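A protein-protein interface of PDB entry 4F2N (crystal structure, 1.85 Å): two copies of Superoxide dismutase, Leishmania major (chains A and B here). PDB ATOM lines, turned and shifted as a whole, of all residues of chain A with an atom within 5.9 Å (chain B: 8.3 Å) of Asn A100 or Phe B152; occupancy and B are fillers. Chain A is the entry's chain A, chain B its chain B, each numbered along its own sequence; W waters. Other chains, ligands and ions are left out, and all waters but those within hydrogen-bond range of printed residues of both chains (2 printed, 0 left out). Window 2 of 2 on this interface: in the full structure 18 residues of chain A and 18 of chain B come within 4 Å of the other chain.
Water W2 lies within hydrogen-bond range of the side-chain amide oxygen of Asn B175 (2.6 Å), the side-chain amide oxygen of Asn A175 (2.7 Å) and the backbone NH of Ser B154 (2.9 Å). Water W1 lies within hydrogen-bond range of OG of Ser B174 (2.7 Å), O of Ser B154 (2.8 Å), O of Phe B152 (2.9 Å) and ND2 of Asn A175 (3.0 Å).
Among the printed residues, pairs that only touch across the chains: Asn A100 with Phe B152, Gln A104 with Phe B152, Asn A175 with Phe B152, Asn A175 with Gly B153, Ala A176 with Phe B152, Trp A193 with Phe B152 and Trp A193 with Gly B153.
Position printed for both chains: 175. Of the 7 pairs that touch across the chains among the printed residues, none has its exchanged pair printed and touching as well.
Of the printed residues of chain B, Asn A100 touches Phe B152. Phe B152 touches just these residues of chain A: Asn A100 (3.3 Å), Gln A104 (3.9 Å), Asn A175 (3.7 Å), Ala A176 (3.8 Å) and Trp A193 (3.7 Å). Of the printed residues of chain B, Asn A175 touches Phe B152 and Gly B153. Printed residues of chain B within 4 Å of Ala A176: Phe B152. Of the printed residues of chain B, Trp A193 touches Phe B152 and Gly B153. Printed residues of chain B within 4 Å of Gln A104: Phe B152 (3.9 Å). Of the printed residues of chain A, Gly B153 touches Asn A175 and Trp A193. Thr B157 touches none of the printed residues of chain A. The nearest residue of chain B that does not touch Asn A100 is Gly B153 (6.9 Å).
OH of Tyr A66 is in hydrogen-bond range of NE2 of Gln A104 (3.1 Å). The backbone carbonyl oxygen (O) of Asn A175 lies within hydrogen-bond range of the indole nitrogen (NE1) of Trp A193 (3.0 Å). NH2 of Arg B205 lies within hydrogen-bond range of O of Gly B153.
Hydrophobic or aromatic side chains of chain A that line the printed part of chain B: Ala A176 and Trp A193. Of the 18 printed residues of chain B, 2 touch a printed residue of chain A. Hydrophobic or aromatic side chains of chain B that line the printed part of chain A: Phe B152.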
ATOM      1  N   TYR A  66     -23.061  -5.551  24.588  1.00  0.00           N
ATOM      2  CA  TYR A  66     -23.975  -5.466  23.441  1.00  0.00           C
ATOM      3  C   TYR A  66     -25.390  -5.888  23.853  1.00  0.00           C
ATOM      4  O   TYR A  66     -26.359  -5.225  23.498  1.00  0.00           O
ATOM      5  CB  TYR A  66     -23.495  -6.329  22.259  1.00  0.00           C
ATOM      6  CG  TYR A  66     -22.203  -5.846  21.637  1.00  0.00           C
ATOM      7  CD1 TYR A  66     -22.091  -4.536  21.116  1.00  0.00           C
ATOM      8  CD2 TYR A  66     -21.107  -6.691  21.546  1.00  0.00           C
ATOM      9  CE1 TYR A  66     -20.901  -4.097  20.559  1.00  0.00           C
ATOM     10  CE2 TYR A  66     -19.918  -6.269  20.983  1.00  0.00           C
ATOM     11  CZ  TYR A  66     -19.817  -4.972  20.494  1.00  0.00           C
ATOM     12  OH  TYR A  66     -18.638  -4.580  19.909  1.00  0.00           O
ATOM     13  N   THR A  89     -33.314  -2.065  11.017  1.00  0.00           N
ATOM     14  CA  THR A  89     -32.512  -0.898  11.359  1.00  0.00           C
ATOM     15  C   THR A  89     -31.343  -0.659  10.405  1.00  0.00           C
ATOM     16  O   THR A  89     -30.715   0.404  10.435  1.00  0.00           O
ATOM     17  CB  THR A  89     -31.939  -1.013  12.775  1.00  0.00           C
ATOM     18  OG1 THR A  89     -31.146  -2.203  12.862  1.00  0.00           O
ATOM     19  CG2 THR A  89     -33.056  -1.053  13.798  1.00  0.00           C
ATOM     20  N   SER A  95     -31.073   4.965  13.382  1.00  0.00           N
ATOM     21  CA  SER A  95     -31.006   3.723  14.157  1.00  0.00           C
ATOM     22  C   SER A  95     -29.637   3.021  14.153  1.00  0.00           C
ATOM     23  O   SER A  95     -29.566   1.818  14.430  1.00  0.00           O
ATOM     24  CB  SER A  95     -32.083   2.745  13.688  1.00  0.00           C
ATOM     25  OG  SER A  95     -33.366   3.259  13.999  1.00  0.00           O
ATOM     26  N   LYS A  96     -28.569   3.766  13.860  1.00  0.00           N
ATOM     27  CA  LYS A  96     -27.197   3.200  13.806  1.00  0.00           C
ATOM     28  C   LYS A  96     -26.754   2.513  15.098  1.00  0.00           C
ATOM     29  O   LYS A  96     -26.154   1.442  15.055  1.00  0.00           O
ATOM     30  CB  LYS A  96     -26.184   4.263  13.371  1.00  0.00           C
ATOM     31  N   VAL A  97     -27.064   3.115  16.246  1.00  0.00           N
ATOM     32  CA  VAL A  97     -26.630   2.549  17.517  1.00  0.00           C
ATOM     33  C   VAL A  97     -27.318   1.204  17.774  1.00  0.00           C
ATOM     34  O   VAL A  97     -26.666   0.246  18.136  1.00  0.00           O
ATOM     35  CB  VAL A  97     -26.812   3.513  18.705  1.00  0.00           C
ATOM     36  CG1 VAL A  97     -26.426   2.829  20.008  1.00  0.00           C
ATOM     37  CG2 VAL A  97     -25.937   4.762  18.507  1.00  0.00           C
ATOM     38  N   MET A  98     -28.628   1.125  17.534  1.00  0.00           N
ATOM     39  CA  MET A  98     -29.333  -0.145  17.749  1.00  0.00           C
ATOM     40  C   MET A  98     -28.893  -1.211  16.746  1.00  0.00           C
ATOM     41  O   MET A  98     -28.706  -2.377  17.111  1.00  0.00           O
ATOM     42  CB  MET A  98     -30.849   0.043  17.731  1.00  0.00           C
ATOM     43  CG  MET A  98     -31.637  -1.245  18.001  1.00  0.00           C
ATOM     44  SD  MET A  98     -33.415  -1.049  18.340  1.00  0.00           S
ATOM     45  CE  MET A  98     -33.915   0.250  17.219  1.00  0.00           C
ATOM     46  N   PHE A  99     -28.715  -0.810  15.490  1.00  0.00           N
ATOM     47  CA  PHE A  99     -28.183  -1.719  14.506  1.00  0.00           C
ATOM     48  C   PHE A  99     -26.870  -2.327  15.008  1.00  0.00           C
ATOM     49  O   PHE A  99     -26.723  -3.539  15.032  1.00  0.00           O
ATOM     50  CB  PHE A  99     -27.950  -1.040  13.154  1.00  0.00           C
ATOM     51  CG  PHE A  99     -27.207  -1.919  12.186  1.00  0.00           C
ATOM     52  CD1 PHE A  99     -27.910  -2.785  11.346  1.00  0.00           C
ATOM     53  CD2 PHE A  99     -25.800  -1.947  12.167  1.00  0.00           C
ATOM     54  CE1 PHE A  99     -27.225  -3.633  10.480  1.00  0.00           C
ATOM     55  CE2 PHE A  99     -25.115  -2.798  11.297  1.00  0.00           C
ATOM     56  CZ  PHE A  99     -25.833  -3.631  10.448  1.00  0.00           C
ATOM     57  N   ASN A 100     -25.937  -1.481  15.419  1.00  0.00           N
ATOM     58  CA  ASN A 100     -24.644  -1.959  15.916  1.00  0.00           C
ATOM     59  C   ASN A 100     -24.797  -2.977  17.049  1.00  0.00           C
ATOM     60  O   ASN A 100     -24.123  -4.010  17.022  1.00  0.00           O
ATOM     61  CB  ASN A 100     -23.726  -0.787  16.305  1.00  0.00           C
ATOM     62  CG  ASN A 100     -23.109  -0.106  15.102  1.00  0.00           C
ATOM     63  OD1 ASN A 100     -23.139  -0.636  13.980  1.00  0.00           O
ATOM     64  ND2 ASN A 100     -22.554   1.095  15.318  1.00  0.00           N
ATOM     65  N   GLN A 101     -25.669  -2.718  18.029  1.00  0.00           N
ATOM     66  CA  GLN A 101     -25.827  -3.655  19.171  1.00  0.00           C
ATOM     67  C   GLN A 101     -26.437  -4.979  18.711  1.00  0.00           C
ATOM     68  O   GLN A 101     -25.925  -6.032  19.023  1.00  0.00           O
ATOM     69  CB  GLN A 101     -26.668  -3.081  20.325  1.00  0.00           C
ATOM     70  CG  GLN A 101     -26.227  -1.689  20.776  1.00  0.00           C
ATOM     71  CD  GLN A 101     -24.758  -1.612  21.112  1.00  0.00           C
ATOM     72  OE1 GLN A 101     -24.266  -2.267  22.042  1.00  0.00           O
ATOM     73  NE2 GLN A 101     -24.038  -0.782  20.371  1.00  0.00           N
ATOM     74  N   ALA A 102     -27.538  -4.904  17.981  1.00  0.00           N
ATOM     75  CA  ALA A 102     -28.230  -6.096  17.504  1.00  0.00           C
ATOM     76  C   ALA A 102     -27.327  -6.942  16.596  1.00  0.00           C
ATOM     77  O   ALA A 102     -27.262  -8.178  16.750  1.00  0.00           O
ATOM     78  CB  ALA A 102     -29.498  -5.701  16.791  1.00  0.00           C
ATOM     79  N   ALA A 103     -26.650  -6.282  15.655  1.00  0.00           N
ATOM     80  CA  ALA A 103     -25.748  -6.967  14.739  1.00  0.00           C
ATOM     81  C   ALA A 103     -24.596  -7.642  15.481  1.00  0.00           C
ATOM     82  O   ALA A 103     -24.289  -8.833  15.217  1.00  0.00           O
ATOM     83  CB  ALA A 103     -25.227  -5.996  13.677  1.00  0.00           C
ATOM     84  N   GLN A 104     -23.994  -6.921  16.439  1.00  0.00           N
ATOM     85  CA  GLN A 104     -22.917  -7.493  17.224  1.00  0.00           C
ATOM     86  C   GLN A 104     -23.393  -8.669  18.106  1.00  0.00           C
ATOM     87  O   GLN A 104     -22.639  -9.618  18.329  1.00  0.00           O
ATOM     88  CB  GLN A 104     -22.186  -6.441  18.083  1.00  0.00           C
ATOM     89  CG  GLN A 104     -21.265  -5.546  17.264  1.00  0.00           C
ATOM     90  CD  GLN A 104     -20.087  -6.324  16.649  1.00  0.00           C
ATOM     91  OE1 GLN A 104     -20.225  -6.971  15.600  1.00  0.00           O
ATOM     92  NE2 GLN A 104     -18.936  -6.255  17.292  1.00  0.00           N
ATOM     93  N   HIS A 105     -24.603  -8.558  18.651  1.00  0.00           N
ATOM     94  CA  HIS A 105     -25.183  -9.647  19.426  1.00  0.00           C
ATOM     95  C   HIS A 105     -25.355 -10.871  18.555  1.00  0.00           C
ATOM     96  O   HIS A 105     -24.908 -11.972  18.916  1.00  0.00           O
ATOM     97  CB  HIS A 105     -26.507  -9.190  20.078  1.00  0.00           C
ATOM     98  CG  HIS A 105     -27.244 -10.296  20.778  1.00  0.00           C
ATOM     99  ND1 HIS A 105     -26.608 -11.248  21.480  1.00  0.00           N
ATOM    100  CD2 HIS A 105     -28.613 -10.578  20.874  1.00  0.00           C
ATOM    101  CE1 HIS A 105     -27.508 -12.104  22.008  1.00  0.00           C
ATOM    102  NE2 HIS A 105     -28.738 -11.693  21.639  1.00  0.00           N
ATOM    103  N   ASN A 175     -16.750  -3.714  11.153  1.00  0.00           N
ATOM    104  CA  ASN A 175     -17.436  -3.299  12.366  1.00  0.00           C
ATOM    105  C   ASN A 175     -18.528  -4.276  12.743  1.00  0.00           C
ATOM    106  O   ASN A 175     -18.205  -5.426  13.027  1.00  0.00           O
ATOM    107  CB  ASN A 175     -17.833  -1.820  12.356  1.00  0.00           C
ATOM    108  CG  ASN A 175     -16.606  -0.909  12.373  1.00  0.00           C
ATOM    109  OD1 ASN A 175     -15.482  -1.394  12.513  1.00  0.00           O
ATOM    110  ND2 ASN A 175     -16.814   0.409  12.190  1.00  0.00           N
ATOM    111  N   ALA A 176     -19.788  -3.863  12.702  1.00  0.00           N
ATOM    112  CA  ALA A 176     -20.865  -4.784  13.077  1.00  0.00           C
ATOM    113  C   ALA A 176     -21.496  -5.412  11.838  1.00  0.00           C
ATOM    114  O   ALA A 176     -22.462  -6.171  11.952  1.00  0.00           O
ATOM    115  CB  ALA A 176     -21.910  -4.034  13.886  1.00  0.00           C
ATOM    116  N   TRP A 193     -12.200  -8.376  15.111  1.00  0.00           N
ATOM    117  CA  TRP A 193     -11.935  -7.328  16.106  1.00  0.00           C
ATOM    118  C   TRP A 193     -10.739  -7.764  16.902  1.00  0.00           C
ATOM    119  O   TRP A 193     -10.621  -8.934  17.232  1.00  0.00           O
ATOM    120  CB  TRP A 193     -13.096  -7.144  17.046  1.00  0.00           C
ATOM    121  CG  TRP A 193     -14.305  -6.438  16.432  1.00  0.00           C
ATOM    122  CD1 TRP A 193     -15.085  -6.833  15.341  1.00  0.00           C
ATOM    123  CD2 TRP A 193     -14.934  -5.216  16.943  1.00  0.00           C
ATOM    124  NE1 TRP A 193     -16.108  -5.930  15.117  1.00  0.00           N
ATOM    125  CE2 TRP A 193     -16.083  -4.944  16.068  1.00  0.00           C
ATOM    126  CE3 TRP A 193     -14.649  -4.342  17.994  1.00  0.00           C
ATOM    127  CZ2 TRP A 193     -16.900  -3.829  16.251  1.00  0.00           C
ATOM    128  CZ3 TRP A 193     -15.497  -3.237  18.197  1.00  0.00           C
ATOM    129  CH2 TRP A 193     -16.597  -2.989  17.336  1.00  0.00           C
ATOM    130  N   GLN B 146     -15.539  11.065  26.128  1.00  0.00           N
ATOM    131  CA  GLN B 146     -16.832  10.568  25.677  1.00  0.00           C
ATOM    132  C   GLN B 146     -16.816  10.247  24.181  1.00  0.00           C
ATOM    133  O   GLN B 146     -17.314   9.210  23.748  1.00  0.00           O
ATOM    134  CB  GLN B 146     -17.926  11.583  26.024  1.00  0.00           C
ATOM    135  CG  GLN B 146     -19.263  11.365  25.330  1.00  0.00           C
ATOM    136  CD  GLN B 146     -20.310  12.328  25.822  1.00  0.00           C
ATOM    137  OE1 GLN B 146     -20.174  12.897  26.912  1.00  0.00           O
ATOM    138  NE2 GLN B 146     -21.352  12.537  25.020  1.00  0.00           N
ATOM    139  N   ALA B 147     -16.236  11.143  23.389  1.00  0.00           N
ATOM    140  CA  ALA B 147     -16.149  10.884  21.941  1.00  0.00           C
ATOM    141  C   ALA B 147     -15.284   9.632  21.661  1.00  0.00           C
ATOM    142  O   ALA B 147     -15.615   8.816  20.787  1.00  0.00           O
ATOM    143  CB  ALA B 147     -15.616  12.108  21.178  1.00  0.00           C
ATOM    144  N   GLY B 148     -14.184   9.483  22.399  1.00  0.00           N
ATOM    145  CA  GLY B 148     -13.338   8.287  22.224  1.00  0.00           C
ATOM    146  C   GLY B 148     -14.058   6.994  22.615  1.00  0.00           C
ATOM    147  O   GLY B 148     -13.940   5.979  21.929  1.00  0.00           O
ATOM    148  N   VAL B 149     -14.784   7.031  23.726  1.00  0.00           N
ATOM    149  CA  VAL B 149     -15.547   5.864  24.190  1.00  0.00           C
ATOM    150  C   VAL B 149     -16.595   5.458  23.141  1.00  0.00           C
ATOM    151  O   VAL B 149     -16.777   4.269  22.853  1.00  0.00           O
ATOM    152  CB  VAL B 149     -16.243   6.169  25.522  1.00  0.00           C
ATOM    153  CG1 VAL B 149     -17.343   5.144  25.821  1.00  0.00           C
ATOM    154  CG2 VAL B 149     -15.196   6.147  26.635  1.00  0.00           C
ATOM    155  N   ASN B 150     -17.257   6.463  22.582  1.00  0.00           N
ATOM    156  CA  ASN B 150     -18.350   6.255  21.651  1.00  0.00           C
ATOM    157  C   ASN B 150     -17.925   5.970  20.218  1.00  0.00           C
ATOM    158  O   ASN B 150     -18.769   5.746  19.376  1.00  0.00           O
ATOM    159  CB  ASN B 150     -19.258   7.479  21.651  1.00  0.00           C
ATOM    160  CG  ASN B 150     -20.042   7.625  22.931  1.00  0.00           C
ATOM    161  OD1 ASN B 150     -20.241   6.674  23.680  1.00  0.00           O
ATOM    162  ND2 ASN B 150     -20.537   8.821  23.158  1.00  0.00           N
ATOM    163  N   ASN B 151     -16.629   6.006  19.930  1.00  0.00           N
ATOM    164  CA  ASN B 151     -16.163   5.795  18.561  1.00  0.00           C
ATOM    165  C   ASN B 151     -16.245   4.295  18.238  1.00  0.00           C
ATOM    166  O   ASN B 151     -15.374   3.522  18.664  1.00  0.00           O
ATOM    167  CB  ASN B 151     -14.734   6.301  18.388  1.00  0.00           C
ATOM    168  CG  ASN B 151     -14.367   6.486  16.945  1.00  0.00           C
ATOM    169  OD1 ASN B 151     -15.231   6.617  16.106  1.00  0.00           O
ATOM    170  ND2 ASN B 151     -13.092   6.578  16.665  1.00  0.00           N
ATOM    171  N   PHE B 152     -17.275   3.886  17.503  1.00  0.00           N
ATOM    172  CA  PHE B 152     -17.548   2.444  17.336  1.00  0.00           C
ATOM    173  C   PHE B 152     -16.463   1.814  16.483  1.00  0.00           C
ATOM    174  O   PHE B 152     -16.179   2.310  15.382  1.00  0.00           O
ATOM    175  CB  PHE B 152     -18.911   2.202  16.662  1.00  0.00           C
ATOM    176  CG  PHE B 152     -19.329   0.760  16.644  1.00  0.00           C
ATOM    177  CD1 PHE B 152     -19.638   0.097  17.827  1.00  0.00           C
ATOM    178  CD2 PHE B 152     -19.418   0.069  15.462  1.00  0.00           C
ATOM    179  CE1 PHE B 152     -20.043  -1.240  17.811  1.00  0.00           C
ATOM    180  CE2 PHE B 152     -19.819  -1.264  15.435  1.00  0.00           C
ATOM    181  CZ  PHE B 152     -20.117  -1.918  16.614  1.00  0.00           C
ATOM    182  N   GLY B 153     -15.875   0.727  16.974  1.00  0.00           N
ATOM    183  CA  GLY B 153     -14.835  -0.017  16.211  1.00  0.00           C
ATOM    184  C   GLY B 153     -13.463   0.589  16.432  1.00  0.00           C
ATOM    185  O   GLY B 153     -13.167   1.144  17.537  1.00  0.00           O
ATOM    186  N   SER B 154     -12.619   0.507  15.407  1.00  0.00           N
ATOM    187  CA  SER B 154     -11.266   1.089  15.492  1.00  0.00           C
ATOM    188  C   SER B 154     -11.276   2.539  15.050  1.00  0.00           C
ATOM    189  O   SER B 154     -12.036   2.910  14.130  1.00  0.00           O
ATOM    190  CB  SER B 154     -10.300   0.329  14.581  1.00  0.00           C
ATOM    191  OG  SER B 154     -10.400  -1.080  14.780  1.00  0.00           O
ATOM    192  N   GLY B 155     -10.425   3.357  15.634  1.00  0.00           N
ATOM    193  CA  GLY B 155     -10.204   4.699  15.052  1.00  0.00           C
ATOM    194  C   GLY B 155      -9.423   5.603  15.972  1.00  0.00           C
ATOM    195  O   GLY B 155      -8.684   5.130  16.837  1.00  0.00           O
ATOM    196  N   TRP B 156      -9.668   6.900  15.819  1.00  0.00           N
ATOM    197  CA  TRP B 156      -8.893   7.969  16.443  1.00  0.00           C
ATOM    198  C   TRP B 156      -9.840   9.050  16.887  1.00  0.00           C
ATOM    199  O   TRP B 156     -10.859   9.349  16.200  1.00  0.00           O
ATOM    200  CB  TRP B 156      -7.891   8.559  15.403  1.00  0.00           C
ATOM    201  CG  TRP B 156      -6.906   7.529  14.903  1.00  0.00           C
ATOM    202  CD1 TRP B 156      -7.084   6.617  13.851  1.00  0.00           C
ATOM    203  CD2 TRP B 156      -5.547   7.272  15.412  1.00  0.00           C
ATOM    204  NE1 TRP B 156      -5.967   5.830  13.691  1.00  0.00           N
ATOM    205  CE2 TRP B 156      -5.017   6.158  14.618  1.00  0.00           C
ATOM    206  CE3 TRP B 156      -4.756   7.827  16.422  1.00  0.00           C
ATOM    207  CZ2 TRP B 156      -3.752   5.663  14.811  1.00  0.00           C
ATOM    208  CZ3 TRP B 156      -3.454   7.297  16.631  1.00  0.00           C
ATOM    209  CH2 TRP B 156      -2.972   6.247  15.842  1.00  0.00           C
ATOM    210  N   THR B 157      -9.506   9.670  18.006  1.00  0.00           N
ATOM    211  CA  THR B 157     -10.218  10.850  18.468  1.00  0.00           C
ATOM    212  C   THR B 157      -9.218  12.025  18.492  1.00  0.00           C
ATOM    213  O   THR B 157      -8.077  11.884  18.966  1.00  0.00           O
ATOM    214  CB  THR B 157     -10.813  10.613  19.863  1.00  0.00           C
ATOM    215  OG1 THR B 157     -11.735   9.527  19.759  1.00  0.00           O
ATOM    216  CG2 THR B 157     -11.579  11.843  20.360  1.00  0.00           C
ATOM    217  N   SER B 172     -13.937  12.584  15.700  1.00  0.00           N
ATOM    218  CA  SER B 172     -13.566  11.165  15.732  1.00  0.00           C
ATOM    219  C   SER B 172     -13.504  10.663  14.318  1.00  0.00           C
ATOM    220  O   SER B 172     -14.345  11.044  13.485  1.00  0.00           O
ATOM    221  CB  SER B 172     -14.613  10.379  16.505  1.00  0.00           C
ATOM    222  OG  SER B 172     -14.393  10.578  17.885  1.00  0.00           O
ATOM    223  N   THR B 173     -12.520   9.815  14.016  1.00  0.00           N
ATOM    224  CA  THR B 173     -12.482   9.171  12.715  1.00  0.00           C
ATOM    225  C   THR B 173     -12.505   7.635  12.901  1.00  0.00           C
ATOM    226  O   THR B 173     -12.187   7.127  13.986  1.00  0.00           O
ATOM    227  CB  THR B 173     -11.235   9.571  11.901  1.00  0.00           C
ATOM    228  OG1 THR B 173     -10.045   9.293  12.680  1.00  0.00           O
ATOM    229  CG2 THR B 173     -11.273  11.101  11.505  1.00  0.00           C
ATOM    230  N   SER B 174     -12.892   6.932  11.850  1.00  0.00           N
ATOM    231  CA  SER B 174     -12.928   5.468  11.843  1.00  0.00           C
ATOM    232  C   SER B 174     -11.638   4.947  11.163  1.00  0.00           C
ATOM    233  O   SER B 174     -11.222   5.476  10.114  1.00  0.00           O
ATOM    234  CB  SER B 174     -14.164   5.013  11.042  1.00  0.00           C
ATOM    235  OG  SER B 174     -14.150   3.610  10.743  1.00  0.00           O
ATOM    236  N   ASN B 175     -11.063   3.889  11.725  1.00  0.00           N
ATOM    237  CA  ASN B 175      -9.967   3.148  11.059  1.00  0.00           C
ATOM    238  C   ASN B 175      -8.738   4.039  10.806  1.00  0.00           C
ATOM    239  O   ASN B 175      -8.126   4.458  11.775  1.00  0.00           O
ATOM    240  CB  ASN B 175     -10.449   2.419   9.793  1.00  0.00           C
ATOM    241  CG  ASN B 175     -11.421   1.277  10.136  1.00  0.00           C
ATOM    242  OD1 ASN B 175     -11.520   0.899  11.304  1.00  0.00           O
ATOM    243  ND2 ASN B 175     -12.141   0.739   9.133  1.00  0.00           N
ATOM    244  N   VAL B 192      -7.771   5.009  19.448  1.00  0.00           N
ATOM    245  CA  VAL B 192      -8.717   4.116  20.118  1.00  0.00           C
ATOM    246  C   VAL B 192      -8.969   2.826  19.327  1.00  0.00           C
ATOM    247  O   VAL B 192      -9.962   2.126  19.546  1.00  0.00           O
ATOM    248  CB  VAL B 192     -10.033   4.799  20.545  1.00  0.00           C
ATOM    249  CG1 VAL B 192      -9.774   5.880  21.587  1.00  0.00           C
ATOM    250  CG2 VAL B 192     -10.684   5.438  19.334  1.00  0.00           C
ATOM    251  N   ARG B 205     -11.691   0.703  27.742  1.00  0.00           N
ATOM    252  CA  ARG B 205     -11.302   1.852  26.936  1.00  0.00           C
ATOM    253  C   ARG B 205     -11.527   3.170  27.693  1.00  0.00           C
ATOM    254  O   ARG B 205     -10.729   4.098  27.569  1.00  0.00           O
ATOM    255  CB  ARG B 205     -12.064   1.872  25.594  1.00  0.00           C
ATOM    256  CG  ARG B 205     -11.573   2.974  24.655  1.00  0.00           C
ATOM    257  CD  ARG B 205     -12.475   3.221  23.465  1.00  0.00           C
ATOM    258  NE  ARG B 205     -12.399   2.160  22.453  1.00  0.00           N
ATOM    259  CZ  ARG B 205     -13.015   2.216  21.261  1.00  0.00           C
ATOM    260  NH1 ARG B 205     -13.703   3.295  20.895  1.00  0.00           N
ATOM    261  NH2 ARG B 205     -12.883   1.206  20.381  1.00  0.00           N
HETATM  262  O   HOH W   1     -14.508   2.202  13.018  1.00  0.00           O
HETATM  263  O   HOH W   2     -12.932  -0.684  12.836  1.00  0.00           O
